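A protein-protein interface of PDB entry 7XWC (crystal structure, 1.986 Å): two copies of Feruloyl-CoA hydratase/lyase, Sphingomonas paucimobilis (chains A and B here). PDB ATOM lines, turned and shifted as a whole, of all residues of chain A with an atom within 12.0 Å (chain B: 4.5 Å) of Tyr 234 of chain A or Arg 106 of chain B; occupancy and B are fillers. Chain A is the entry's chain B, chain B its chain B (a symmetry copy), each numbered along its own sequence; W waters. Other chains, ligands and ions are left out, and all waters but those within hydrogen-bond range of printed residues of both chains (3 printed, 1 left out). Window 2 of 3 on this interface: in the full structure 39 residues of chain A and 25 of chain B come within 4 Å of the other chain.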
ATOM      1  N   ALA A 225      -4.818  -2.916  12.015  1.00  0.00           N
ATOM      2  CA  ALA A 225      -5.550  -1.741  12.538  1.00  0.00           C
ATOM      3  C   ALA A 225      -4.543  -0.814  13.230  1.00  0.00           C
ATOM      4  O   ALA A 225      -4.578   0.391  12.976  1.00  0.00           O
ATOM      5  CB  ALA A 225      -6.682  -2.178  13.449  1.00  0.00           C
ATOM      6  N   VAL A 226      -3.617  -1.348  14.022  1.00  0.00           N
ATOM      7  CA  VAL A 226      -2.585  -0.502  14.668  1.00  0.00           C
ATOM      8  C   VAL A 226      -1.829   0.309  13.591  1.00  0.00           C
ATOM      9  O   VAL A 226      -1.579   1.513  13.860  1.00  0.00           O
ATOM     10  CB  VAL A 226      -1.643  -1.349  15.540  1.00  0.00           C
ATOM     11  CG1 VAL A 226      -0.483  -0.528  16.061  1.00  0.00           C
ATOM     12  CG2 VAL A 226      -2.397  -2.017  16.676  1.00  0.00           C
ATOM     13  N   ARG A 228      -2.580   1.048  10.425  1.00  0.00           N
ATOM     14  CA  ARG A 228      -3.480   1.896   9.633  1.00  0.00           C
ATOM     15  C   ARG A 228      -3.905   3.134  10.441  1.00  0.00           C
ATOM     16  O   ARG A 228      -3.880   4.237   9.858  1.00  0.00           O
ATOM     17  CB  ARG A 228      -4.696   1.069   9.183  1.00  0.00           C
ATOM     18  CG  ARG A 228      -4.420   0.071   8.072  1.00  0.00           C
ATOM     19  CD  ARG A 228      -4.288   0.681   6.674  1.00  0.00           C
ATOM     20  NE  ARG A 228      -3.892  -0.364   5.721  1.00  0.00           N
ATOM     21  CZ  ARG A 228      -3.358  -0.177   4.496  1.00  0.00           C
ATOM     22  NH1 ARG A 228      -3.132   1.024   4.008  1.00  0.00           N
ATOM     23  NH2 ARG A 228      -2.974  -1.220   3.787  1.00  0.00           N
ATOM     24  N   VAL A 229      -4.316   3.012  11.707  1.00  0.00           N
ATOM     25  CA  VAL A 229      -4.928   4.162  12.441  1.00  0.00           C
ATOM     26  C   VAL A 229      -3.845   5.173  12.828  1.00  0.00           C
ATOM     27  O   VAL A 229      -4.186   6.338  13.047  1.00  0.00           O
ATOM     28  CB  VAL A 229      -5.794   3.773  13.654  1.00  0.00           C
ATOM     29  CG1 VAL A 229      -6.925   2.885  13.200  1.00  0.00           C
ATOM     30  CG2 VAL A 229      -5.012   3.137  14.765  1.00  0.00           C
ATOM     31  N   LYS A 230      -2.589   4.764  12.786  1.00  0.00           N
ATOM     32  CA  LYS A 230      -1.448   5.699  12.830  1.00  0.00           C
ATOM     33  C   LYS A 230      -1.578   6.811  11.776  1.00  0.00           C
ATOM     34  O   LYS A 230      -1.068   7.880  12.036  1.00  0.00           O
ATOM     35  CB  LYS A 230      -0.139   4.937  12.656  1.00  0.00           C
ATOM     36  CG  LYS A 230       1.090   5.835  12.688  1.00  0.00           C
ATOM     37  CD  LYS A 230       1.393   6.314  14.067  1.00  0.00           C
ATOM     38  CE  LYS A 230       2.287   5.321  14.787  1.00  0.00           C
ATOM     39  NZ  LYS A 230       3.660   5.373  14.220  1.00  0.00           N
ATOM     40  N   GLU A 231      -2.228   6.603  10.635  1.00  0.00           N
ATOM     41  CA  GLU A 231      -2.250   7.591   9.529  1.00  0.00           C
ATOM     42  C   GLU A 231      -3.666   8.101   9.304  1.00  0.00           C
ATOM     43  O   GLU A 231      -4.008   8.424   8.139  1.00  0.00           O
ATOM     44  CB  GLU A 231      -1.694   6.975   8.235  1.00  0.00           C
ATOM     45  CG  GLU A 231      -0.216   6.592   8.390  1.00  0.00           C
ATOM     46  CD  GLU A 231       0.495   6.028   7.163  1.00  0.00           C
ATOM     47  OE1 GLU A 231      -0.203   5.684   6.140  1.00  0.00           O
ATOM     48  OE2 GLU A 231       1.734   6.025   7.218  1.00  0.00           O
ATOM     49  N   MET A 232      -4.485   8.108  10.349  1.00  0.00           N
ATOM     50  CA  MET A 232      -5.842   8.692  10.275  1.00  0.00           C
ATOM     51  C   MET A 232      -6.032   9.674  11.431  1.00  0.00           C
ATOM     52  O   MET A 232      -5.355   9.510  12.505  1.00  0.00           O
ATOM     53  CB  MET A 232      -6.895   7.599  10.369  1.00  0.00           C
ATOM     54  CG  MET A 232      -6.637   6.462   9.433  1.00  0.00           C
ATOM     55  SD  MET A 232      -7.961   5.283   9.645  1.00  0.00           S
ATOM     56  CE  MET A 232      -7.289   4.019   8.587  1.00  0.00           C
ATOM     57  N   THR A 233      -6.966  10.594  11.262  1.00  0.00           N
ATOM     58  CA  THR A 233      -7.494  11.421  12.384  1.00  0.00           C
ATOM     59  C   THR A 233      -8.249  10.503  13.351  1.00  0.00           C
ATOM     60  O   THR A 233      -8.783   9.471  12.915  1.00  0.00           O
ATOM     61  CB  THR A 233      -8.361  12.584  11.912  1.00  0.00           C
ATOM     62  OG1 THR A 233      -9.515  11.918  11.403  1.00  0.00           O
ATOM     63  CG2 THR A 233      -7.619  13.482  10.925  1.00  0.00           C
ATOM     64  N   TYR A 234      -8.300  10.865  14.615  1.00  0.00           N
ATOM     65  CA  TYR A 234      -9.095  10.136  15.623  1.00  0.00           C
ATOM     66  C   TYR A 234     -10.515   9.899  15.089  1.00  0.00           C
ATOM     67  O   TYR A 234     -10.993   8.770  15.183  1.00  0.00           O
ATOM     68  CB  TYR A 234      -9.106  10.856  16.964  1.00  0.00           C
ATOM     69  CG  TYR A 234      -9.652  10.019  18.096  1.00  0.00           C
ATOM     70  CD1 TYR A 234     -11.007   9.859  18.338  1.00  0.00           C
ATOM     71  CD2 TYR A 234      -8.780   9.383  18.968  1.00  0.00           C
ATOM     72  CE1 TYR A 234     -11.488   9.061  19.381  1.00  0.00           C
ATOM     73  CE2 TYR A 234      -9.249   8.593  20.010  1.00  0.00           C
ATOM     74  CZ  TYR A 234     -10.598   8.471  20.261  1.00  0.00           C
ATOM     75  OH  TYR A 234     -10.997   7.684  21.321  1.00  0.00           O
ATOM     76  N   ASP A 235     -11.165  10.915  14.527  1.00  0.00           N
ATOM     77  CA  ASP A 235     -12.585  10.816  14.128  1.00  0.00           C
ATOM     78  C   ASP A 235     -12.713   9.792  12.983  1.00  0.00           C
ATOM     79  O   ASP A 235     -13.694   8.991  13.010  1.00  0.00           O
ATOM     80  CB  ASP A 235     -13.128  12.192  13.767  1.00  0.00           C
ATOM     81  CG  ASP A 235     -14.600  12.176  13.426  1.00  0.00           C
ATOM     82  OD1 ASP A 235     -15.367  11.922  14.366  1.00  0.00           O
ATOM     83  OD2 ASP A 235     -14.966  12.461  12.214  1.00  0.00           O
ATOM     84  N   ASN A 236     -11.775   9.781  12.029  1.00  0.00           N
ATOM     85  CA  ASN A 236     -11.794   8.816  10.899  1.00  0.00           C
ATOM     86  C   ASN A 236     -11.429   7.425  11.412  1.00  0.00           C
ATOM     87  O   ASN A 236     -11.954   6.455  10.878  1.00  0.00           O
ATOM     88  CB  ASN A 236     -10.914   9.250   9.735  1.00  0.00           C
ATOM     89  CG  ASN A 236     -11.553  10.351   8.933  1.00  0.00           C
ATOM     90  OD1 ASN A 236     -12.761  10.512   8.931  1.00  0.00           O
ATOM     91  ND2 ASN A 236     -10.749  11.228   8.387  1.00  0.00           N
ATOM     92  N   ALA A 237     -10.549   7.324  12.404  1.00  0.00           N
ATOM     93  CA  ALA A 237     -10.091   6.035  12.940  1.00  0.00           C
ATOM     94  C   ALA A 237     -11.262   5.316  13.616  1.00  0.00           C
ATOM     95  O   ALA A 237     -11.338   4.073  13.497  1.00  0.00           O
ATOM     96  CB  ALA A 237      -8.953   6.238  13.908  1.00  0.00           C
ATOM     97  N   GLU A 238     -12.148   6.048  14.296  1.00  0.00           N
ATOM     98  CA  GLU A 238     -13.319   5.445  14.992  1.00  0.00           C
ATOM     99  C   GLU A 238     -14.191   4.754  13.941  1.00  0.00           C
ATOM    100  O   GLU A 238     -14.582   3.609  14.195  1.00  0.00           O
ATOM    101  CB  GLU A 238     -14.182   6.455  15.753  1.00  0.00           C
ATOM    102  CG  GLU A 238     -13.664   6.765  17.166  1.00  0.00           C
ATOM    103  CD  GLU A 238     -14.585   7.725  17.917  1.00  0.00           C
ATOM    104  OE1 GLU A 238     -14.565   7.777  19.162  1.00  0.00           O
ATOM    105  OE2 GLU A 238     -15.355   8.391  17.239  1.00  0.00           O
ATOM    106  N   ASP A 239     -14.567   5.459  12.861  1.00  0.00           N
ATOM    107  CA  ASP A 239     -15.496   4.860  11.872  1.00  0.00           C
ATOM    108  C   ASP A 239     -14.800   3.659  11.211  1.00  0.00           C
ATOM    109  O   ASP A 239     -15.484   2.614  11.057  1.00  0.00           O
ATOM    110  CB  ASP A 239     -16.012   5.843  10.833  1.00  0.00           C
ATOM    111  CG  ASP A 239     -17.121   5.194  10.023  1.00  0.00           C
ATOM    112  OD1 ASP A 239     -18.260   5.163  10.572  1.00  0.00           O
ATOM    113  OD2 ASP A 239     -16.818   4.610   8.911  1.00  0.00           O
ATOM    114  N   TYR A 240     -13.501   3.788  10.892  1.00  0.00           N
ATOM    115  CA  TYR A 240     -12.676   2.752  10.241  1.00  0.00           C
ATOM    116  C   TYR A 240     -12.682   1.454  11.061  1.00  0.00           C
ATOM    117  O   TYR A 240     -12.844   0.362  10.471  1.00  0.00           O
ATOM    118  CB  TYR A 240     -11.233   3.225  10.071  1.00  0.00           C
ATOM    119  CG  TYR A 240     -10.277   2.279   9.415  1.00  0.00           C
ATOM    120  CD1 TYR A 240     -10.383   2.005   8.065  1.00  0.00           C
ATOM    121  CD2 TYR A 240      -9.262   1.652  10.107  1.00  0.00           C
ATOM    122  CE1 TYR A 240      -9.476   1.180   7.423  1.00  0.00           C
ATOM    123  CE2 TYR A 240      -8.395   0.754   9.497  1.00  0.00           C
ATOM    124  CZ  TYR A 240      -8.505   0.523   8.140  1.00  0.00           C
ATOM    125  OH  TYR A 240      -7.664  -0.301   7.459  1.00  0.00           O
ATOM    126  N   LEU A 241     -12.345   1.550  12.344  1.00  0.00           N
ATOM    127  CA  LEU A 241     -12.303   0.373  13.251  1.00  0.00           C
ATOM    128  C   LEU A 241     -13.648  -0.366  13.303  1.00  0.00           C
ATOM    129  O   LEU A 241     -13.617  -1.603  13.335  1.00  0.00           O
ATOM    130  CB  LEU A 241     -11.848   0.855  14.624  1.00  0.00           C
ATOM    131  CG  LEU A 241     -10.417   1.378  14.659  1.00  0.00           C
ATOM    132  CD1 LEU A 241     -10.089   2.097  15.943  1.00  0.00           C
ATOM    133  CD2 LEU A 241      -9.446   0.258  14.474  1.00  0.00           C
ATOM    134  N   ILE A 242     -14.788   0.309  13.171  1.00  0.00           N
ATOM    135  CA  ILE A 242     -16.110  -0.359  13.071  1.00  0.00           C
ATOM    136  C   ILE A 242     -16.206  -1.120  11.745  1.00  0.00           C
ATOM    137  O   ILE A 242     -16.688  -2.275  11.766  1.00  0.00           O
ATOM    138  CB  ILE A 242     -17.250   0.649  13.263  1.00  0.00           C
ATOM    139  CG1 ILE A 242     -17.175   1.296  14.651  1.00  0.00           C
ATOM    140  CG2 ILE A 242     -18.610   0.001  13.026  1.00  0.00           C
ATOM    141  CD1 ILE A 242     -18.224   2.341  14.852  1.00  0.00           C
ATOM    142  N   ARG A 243     -15.849  -0.477  10.633  1.00  0.00           N
ATOM    143  CA  ARG A 243     -15.790  -1.100   9.286  1.00  0.00           C
ATOM    144  C   ARG A 243     -14.840  -2.317   9.341  1.00  0.00           C
ATOM    145  O   ARG A 243     -15.196  -3.347   8.804  1.00  0.00           O
ATOM    146  CB  ARG A 243     -15.334  -0.091   8.216  1.00  0.00           C
ATOM    147  CG  ARG A 243     -16.241   1.108   7.995  1.00  0.00           C
ATOM    148  CD  ARG A 243     -17.586   0.838   7.368  1.00  0.00           C
ATOM    149  NE  ARG A 243     -18.604   0.399   8.316  1.00  0.00           N
ATOM    150  CZ  ARG A 243     -19.174   1.176   9.255  1.00  0.00           C
ATOM    151  NH1 ARG A 243     -18.840   2.450   9.385  1.00  0.00           N
ATOM    152  NH2 ARG A 243     -20.064   0.674  10.092  1.00  0.00           N
ATOM    153  N   TRP B 102     -18.369   9.707  25.114  1.00  0.00           N
ATOM    154  CA  TRP B 102     -16.886   9.813  25.027  1.00  0.00           C
ATOM    155  C   TRP B 102     -16.514  11.123  24.326  1.00  0.00           C
ATOM    156  O   TRP B 102     -15.628  11.816  24.811  1.00  0.00           O
ATOM    157  CB  TRP B 102     -16.282   8.618  24.331  1.00  0.00           C
ATOM    158  CG  TRP B 102     -16.680   7.322  24.931  1.00  0.00           C
ATOM    159  CD1 TRP B 102     -17.086   7.064  26.212  1.00  0.00           C
ATOM    160  CD2 TRP B 102     -16.671   6.069  24.236  1.00  0.00           C
ATOM    161  NE1 TRP B 102     -17.330   5.718  26.365  1.00  0.00           N
ATOM    162  CE2 TRP B 102     -17.093   5.086  25.162  1.00  0.00           C
ATOM    163  CE3 TRP B 102     -16.378   5.705  22.917  1.00  0.00           C
ATOM    164  CZ2 TRP B 102     -17.206   3.740  24.799  1.00  0.00           C
ATOM    165  CZ3 TRP B 102     -16.524   4.388  22.557  1.00  0.00           C
ATOM    166  CH2 TRP B 102     -16.932   3.418  23.492  1.00  0.00           C
ATOM    167  N   GLU B 103     -17.203  11.477  23.250  1.00  0.00           N
ATOM    168  CA  GLU B 103     -16.876  12.713  22.495  1.00  0.00           C
ATOM    169  C   GLU B 103     -17.201  13.959  23.335  1.00  0.00           C
ATOM    170  O   GLU B 103     -16.449  14.933  23.290  1.00  0.00           O
ATOM    171  CB  GLU B 103     -17.637  12.723  21.158  1.00  0.00           C
ATOM    172  CG  GLU B 103     -17.205  13.866  20.271  1.00  0.00           C
ATOM    173  CD  GLU B 103     -17.905  13.956  18.916  1.00  0.00           C
ATOM    174  OE1 GLU B 103     -19.138  14.066  18.919  1.00  0.00           O
ATOM    175  OE2 GLU B 103     -17.203  14.006  17.856  1.00  0.00           O
ATOM    176  N   ARG B 104     -18.336  13.997  24.028  1.00  0.00           N
ATOM    177  CA  ARG B 104     -18.704  15.161  24.854  1.00  0.00           C
ATOM    178  C   ARG B 104     -17.614  15.317  25.920  1.00  0.00           C
ATOM    179  O   ARG B 104     -17.218  16.445  26.209  1.00  0.00           O
ATOM    180  CB  ARG B 104     -20.106  14.952  25.442  1.00  0.00           C
ATOM    181  CG  ARG B 104     -20.438  15.880  26.614  1.00  0.00           C
ATOM    182  CD  ARG B 104     -21.599  16.811  26.355  1.00  0.00           C
ATOM    183  NE  ARG B 104     -22.046  16.889  24.978  1.00  0.00           N
ATOM    184  CZ  ARG B 104     -23.296  16.677  24.571  1.00  0.00           C
ATOM    185  NH1 ARG B 104     -24.257  16.347  25.407  1.00  0.00           N
ATOM    186  NH2 ARG B 104     -23.612  16.817  23.313  1.00  0.00           N
ATOM    187  N   LEU B 105     -17.121  14.220  26.473  1.00  0.00           N
ATOM    188  CA  LEU B 105     -16.047  14.280  27.532  1.00  0.00           C
ATOM    189  C   LEU B 105     -14.722  14.766  26.919  1.00  0.00           C
ATOM    190  O   LEU B 105     -14.097  15.643  27.451  1.00  0.00           O
ATOM    191  CB  LEU B 105     -15.868  12.893  28.135  1.00  0.00           C
ATOM    192  CG  LEU B 105     -14.899  12.860  29.311  1.00  0.00           C
ATOM    193  CD1 LEU B 105     -15.379  13.808  30.405  1.00  0.00           C
ATOM    194  CD2 LEU B 105     -14.785  11.457  29.816  1.00  0.00           C
ATOM    195  N   ARG B 106     -14.398  14.293  25.726  1.00  0.00           N
ATOM    196  CA  ARG B 106     -13.116  14.586  25.041  1.00  0.00           C
ATOM    197  C   ARG B 106     -13.032  16.089  24.732  1.00  0.00           C
ATOM    198  O   ARG B 106     -11.967  16.642  24.868  1.00  0.00           O
ATOM    199  CB  ARG B 106     -13.035  13.688  23.795  1.00  0.00           C
ATOM    200  CG  ARG B 106     -11.689  13.736  23.080  1.00  0.00           C
ATOM    201  CD  ARG B 106     -11.464  12.509  22.209  1.00  0.00           C
ATOM    202  NE  ARG B 106     -12.458  12.467  21.173  1.00  0.00           N
ATOM    203  CZ  ARG B 106     -13.454  11.603  21.037  1.00  0.00           C
ATOM    204  NH1 ARG B 106     -13.667  10.597  21.883  1.00  0.00           N
ATOM    205  NH2 ARG B 106     -14.213  11.747  19.972  1.00  0.00           N
ATOM    206  N   TRP B 107     -14.154  16.722  24.372  1.00  0.00           N
ATOM    207  CA  TRP B 107     -14.205  18.158  24.059  1.00  0.00           C
ATOM    208  C   TRP B 107     -14.848  18.940  25.211  1.00  0.00           C
ATOM    209  O   TRP B 107     -15.300  20.055  24.985  1.00  0.00           O
ATOM    210  CB  TRP B 107     -14.886  18.346  22.701  1.00  0.00           C
ATOM    211  CG  TRP B 107     -14.041  17.657  21.679  1.00  0.00           C
ATOM    212  CD1 TRP B 107     -14.317  16.475  21.058  1.00  0.00           C
ATOM    213  CD2 TRP B 107     -12.730  18.064  21.209  1.00  0.00           C
ATOM    214  NE1 TRP B 107     -13.270  16.124  20.241  1.00  0.00           N
ATOM    215  CE2 TRP B 107     -12.282  17.070  20.309  1.00  0.00           C
ATOM    216  CE3 TRP B 107     -11.863  19.126  21.497  1.00  0.00           C
ATOM    217  CZ2 TRP B 107     -11.038  17.133  19.659  1.00  0.00           C
ATOM    218  CZ3 TRP B 107     -10.642  19.185  20.845  1.00  0.00           C
ATOM    219  CH2 TRP B 107     -10.248  18.218  19.920  1.00  0.00           C
ATOM    220  N   TYR B 108     -14.759  18.445  26.445  1.00  0.00           N
ATOM    221  CA  TYR B 108     -15.480  19.065  27.578  1.00  0.00           C
ATOM    222  C   TYR B 108     -15.051  20.520  27.769  1.00  0.00           C
ATOM    223  O   TYR B 108     -13.871  20.842  27.657  1.00  0.00           O
ATOM    224  CB  TYR B 108     -15.247  18.288  28.869  1.00  0.00           C
ATOM    225  CG  TYR B 108     -16.409  18.317  29.829  1.00  0.00           C
ATOM    226  CD1 TYR B 108     -17.651  17.816  29.449  1.00  0.00           C
ATOM    227  CD2 TYR B 108     -16.248  18.746  31.147  1.00  0.00           C
ATOM    228  CE1 TYR B 108     -18.707  17.749  30.338  1.00  0.00           C
ATOM    229  CE2 TYR B 108     -17.289  18.672  32.053  1.00  0.00           C
ATOM    230  CZ  TYR B 108     -18.531  18.194  31.648  1.00  0.00           C
ATOM    231  OH  TYR B 108     -19.590  18.159  32.527  1.00  0.00           O
ATOM    232  N   GLY B 126     -11.670   4.642  25.442  1.00  0.00           N
ATOM    233  CA  GLY B 126     -12.360   5.860  24.968  1.00  0.00           C
ATOM    234  C   GLY B 126     -12.446   6.909  26.069  1.00  0.00           C
ATOM    235  O   GLY B 126     -11.884   8.005  25.966  1.00  0.00           O
ATOM    236  N   PHE B 129      -8.902   8.202  27.233  1.00  0.00           N
ATOM    237  CA  PHE B 129      -8.338   9.179  26.259  1.00  0.00           C
ATOM    238  C   PHE B 129      -9.110  10.507  26.335  1.00  0.00           C
ATOM    239  O   PHE B 129      -8.536  11.601  26.175  1.00  0.00           O
ATOM    240  CB  PHE B 129      -8.388   8.559  24.856  1.00  0.00           C
ATOM    241  CG  PHE B 129      -7.750   9.434  23.816  1.00  0.00           C
ATOM    242  CD1 PHE B 129      -6.388   9.394  23.614  1.00  0.00           C
ATOM    243  CD2 PHE B 129      -8.518  10.305  23.052  1.00  0.00           C
ATOM    244  CE1 PHE B 129      -5.795  10.169  22.626  1.00  0.00           C
ATOM    245  CE2 PHE B 129      -7.915  11.124  22.107  1.00  0.00           C
ATOM    246  CZ  PHE B 129      -6.550  11.065  21.911  1.00  0.00           C
ATOM    247  N   ALA B 130     -10.418  10.434  26.550  1.00  0.00           N
ATOM    248  CA  ALA B 130     -11.306  11.628  26.568  1.00  0.00           C
ATOM    249  C   ALA B 130     -10.975  12.533  27.775  1.00  0.00           C
ATOM    250  O   ALA B 130     -11.237  13.735  27.702  1.00  0.00           O
ATOM    251  CB  ALA B 130     -12.743  11.226  26.570  1.00  0.00           C
ATOM    252  N   ASP B 132      -8.328  14.625  29.833  1.00  0.00           N
ATOM    253  CA  ASP B 132      -7.140  15.371  29.392  1.00  0.00           C
ATOM    254  C   ASP B 132      -5.922  14.791  30.119  1.00  0.00           C
ATOM    255  O   ASP B 132      -4.858  14.655  29.495  1.00  0.00           O
ATOM    256  CB  ASP B 132      -7.343  16.864  29.612  1.00  0.00           C
ATOM    257  CG  ASP B 132      -8.616  17.394  28.985  1.00  0.00           C
ATOM    258  OD1 ASP B 132      -8.904  16.986  27.842  1.00  0.00           O
ATOM    259  OD2 ASP B 132      -9.325  18.218  29.662  1.00  0.00           O
ATOM    260  N   LYS B 159      -6.985   3.149  18.396  1.00  0.00           N
ATOM    261  CA  LYS B 159      -6.530   4.520  18.058  1.00  0.00           C
ATOM    262  C   LYS B 159      -6.019   5.181  19.350  1.00  0.00           C
ATOM    263  O   LYS B 159      -5.011   5.843  19.263  1.00  0.00           O
ATOM    264  CB  LYS B 159      -7.650   5.306  17.404  1.00  0.00           C
ATOM    265  CG  LYS B 159      -7.275   6.746  17.090  1.00  0.00           C
ATOM    266  CD  LYS B 159      -5.968   6.916  16.327  1.00  0.00           C
ATOM    267  CE  LYS B 159      -5.935   8.236  15.549  1.00  0.00           C
ATOM    268  NZ  LYS B 159      -4.620   8.532  14.886  1.00  0.00           N
ATOM    269  N   VAL B 160      -6.636   4.894  20.510  1.00  0.00           N
ATOM    270  CA  VAL B 160      -6.194   5.455  21.828  1.00  0.00           C
ATOM    271  C   VAL B 160      -4.767   4.973  22.103  1.00  0.00           C
ATOM    272  O   VAL B 160      -3.902   5.806  22.505  1.00  0.00           O
ATOM    273  CB  VAL B 160      -7.173   5.077  22.963  1.00  0.00           C
ATOM    274  CG1 VAL B 160      -6.610   5.438  24.338  1.00  0.00           C
ATOM    275  CG2 VAL B 160      -8.574   5.663  22.793  1.00  0.00           C
ATOM    276  N   ASP B 163      -2.316   6.732  19.670  1.00  0.00           N
ATOM    277  CA  ASP B 163      -2.116   8.193  19.891  1.00  0.00           C
ATOM    278  C   ASP B 163      -1.384   8.461  21.211  1.00  0.00           C
ATOM    279  O   ASP B 163      -0.763   9.525  21.299  1.00  0.00           O
ATOM    280  CB  ASP B 163      -3.433   8.967  19.776  1.00  0.00           C
ATOM    281  CG  ASP B 163      -3.858   9.187  18.323  1.00  0.00           C
ATOM    282  OD1 ASP B 163      -3.239   8.549  17.438  1.00  0.00           O
ATOM    283  OD2 ASP B 163      -4.821   9.983  18.072  1.00  0.00           O
ATOM    284  N   ARG B 227      -4.845  18.897  21.651  1.00  0.00           N
ATOM    285  CA  ARG B 227      -5.573  17.764  21.015  1.00  0.00           C
ATOM    286  C   ARG B 227      -5.608  18.042  19.508  1.00  0.00           C
ATOM    287  O   ARG B 227      -5.367  17.151  18.755  1.00  0.00           O
ATOM    288  CB  ARG B 227      -7.011  17.627  21.540  1.00  0.00           C
ATOM    289  CG  ARG B 227      -7.112  17.098  22.960  1.00  0.00           C
ATOM    290  CD  ARG B 227      -8.545  16.891  23.417  1.00  0.00           C
ATOM    291  NE  ARG B 227      -8.599  16.302  24.746  1.00  0.00           N
ATOM    292  CZ  ARG B 227      -8.460  15.032  25.033  1.00  0.00           C
ATOM    293  NH1 ARG B 227      -8.202  14.161  24.080  1.00  0.00           N
ATOM    294  NH2 ARG B 227      -8.497  14.650  26.304  1.00  0.00           N
ATOM    295  N   GLU B 231      -3.094  16.921  14.940  1.00  0.00           N
ATOM    296  CA  GLU B 231      -3.592  16.477  13.615  1.00  0.00           C
ATOM    297  C   GLU B 231      -3.396  17.578  12.581  1.00  0.00           C
ATOM    298  O   GLU B 231      -4.226  17.672  11.643  1.00  0.00           O
ATOM    299  CB  GLU B 231      -5.073  16.078  13.693  1.00  0.00           C
ATOM    300  CG  GLU B 231      -5.276  14.868  14.614  1.00  0.00           C
ATOM    301  CD  GLU B 231      -6.691  14.311  14.740  1.00  0.00           C
ATOM    302  OE1 GLU B 231      -7.675  14.993  14.272  1.00  0.00           O
ATOM    303  OE2 GLU B 231      -6.777  13.171  15.222  1.00  0.00           O
HETATM  304  O   HOH W   1     -16.146   9.342  20.553  1.00  0.00           O
HETATM  305  O   HOH W   2     -11.724   9.271  23.567  1.00  0.00           O
HETATM  306  O   HOH W   3     -10.030  13.595  14.774  1.00  0.00           O
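The backbone NH of Tyr 234 of chain A sits at hydrogen-bond distance from the side-chain carboxylate of Glu 231 of chain B, 2.8 Å away.
The side-chain amino group (NZ) of Lys 159 of chain B lies within hydrogen-bond range of the backbone carbonyl oxygen (O) of Met 232 of chain A, at 2.7 Å.
The backbone carbonyl oxygen (O) of Val 229 of chain A sits at hydrogen-bond distance from the side-chain amino group (NZ) of Lys 159 of chain B, 2.9 Å away.
The side-chain amino group of Lys 159 of chain B lies within salt-bridge range of the side-chain carboxylate of Asp 163 of chain B (2.9 Å).
O of Arg 106 of chain B lies within hydrogen-bond range of NE of Arg 227 of chain B (3.4 Å).
OG1 of Thr 233 of chain A sits at hydrogen-bond distance from N of Asn 236 of chain A.
The backbone carbonyl oxygen (O) of Phe 129 of chain B sits at hydrogen-bond distance from the guanidinium group (NH2) of Arg 227 of chain B (3.1 Å).
Among the printed residues, pairs that only touch across the chains: Thr 233 of chain A with Lys 159 of chain B (3.9 Å), Thr 233 of chain A with Glu 231 of chain B (3.4 Å), Tyr 234 of chain A with Arg 106 of chain B (3.6 Å), Tyr 234 of chain A with Phe 129 of chain B (3.5 Å), Tyr 234 of chain A with Lys 159 of chain B (3.6 Å), Tyr 234 of chain A with Val 160 of chain B (3.5 Å) and Ala 237 of chain A with Lys 159 of chain B (3.6 Å).
Of the printed residues of chain B, Val 229 of chain A touches Lys 159 (2.9 Å).
Of the printed residues of chain B, Met 232 of chain A touches Lys 159 (2.7 Å).
Of the printed residues of chain B, Tyr 234 of chain A touches Arg 106 (3.6 Å), Phe 129 (3.5 Å), Lys 159 (3.6 Å), Val 160 (3.5 Å) and Glu 231 (2.8 Å).
No residue of chain A comes within 4 Å of Leu 105 of chain B.
No residue of chain A comes within 4 Å of Trp 107 of chain B.
No residue of chain A comes within 4 Å of Gly 126 of chain B.
Of chain A, only Tyr 234 (3.5 Å) comes within 4 Å of Val 160 of chain B.
Of the printed residues of chain A, Glu 231 of chain B touches Thr 233 (3.4 Å) and Tyr 234 (2.8 Å).
The nearest residue of chain B that does not touch Tyr 234 of chain A is Asp 163 of chain B (4.1 Å).
The nearest residue of chain A that does not touch Arg 106 of chain B is Glu 238 of chain A (4.02 Å).
Of the 16 printed residues of chain B, 5 touch a printed residue of chain A.
Printed residues of chain B that touch a printed residue of chain A: Arg 106, Phe 129, Lys 159, Val 160 and Glu 231.
Hydrophobic or aromatic side chains of chain B that line the printed part of chain A: Phe 129 and Val 160.
Along chain B the printed residues that touch a printed residue of chain A span positions 106 to 231.
Among the printed residues, 10 pairs touch across the chains.
Position printed for both chains: 231.
Water W2 lies within hydrogen-bond range of the backbone carbonyl oxygen (O) of Gly 126 of chain B (2.7 Å), the side-chain hydroxyl (OH) of Tyr 234 of chain A (2.8 Å), the guanidinium group (NH1) of Arg 106 of chain B (2.9 Å) and the backbone NH (N) of Ala 130 of chain B (3.5 Å).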
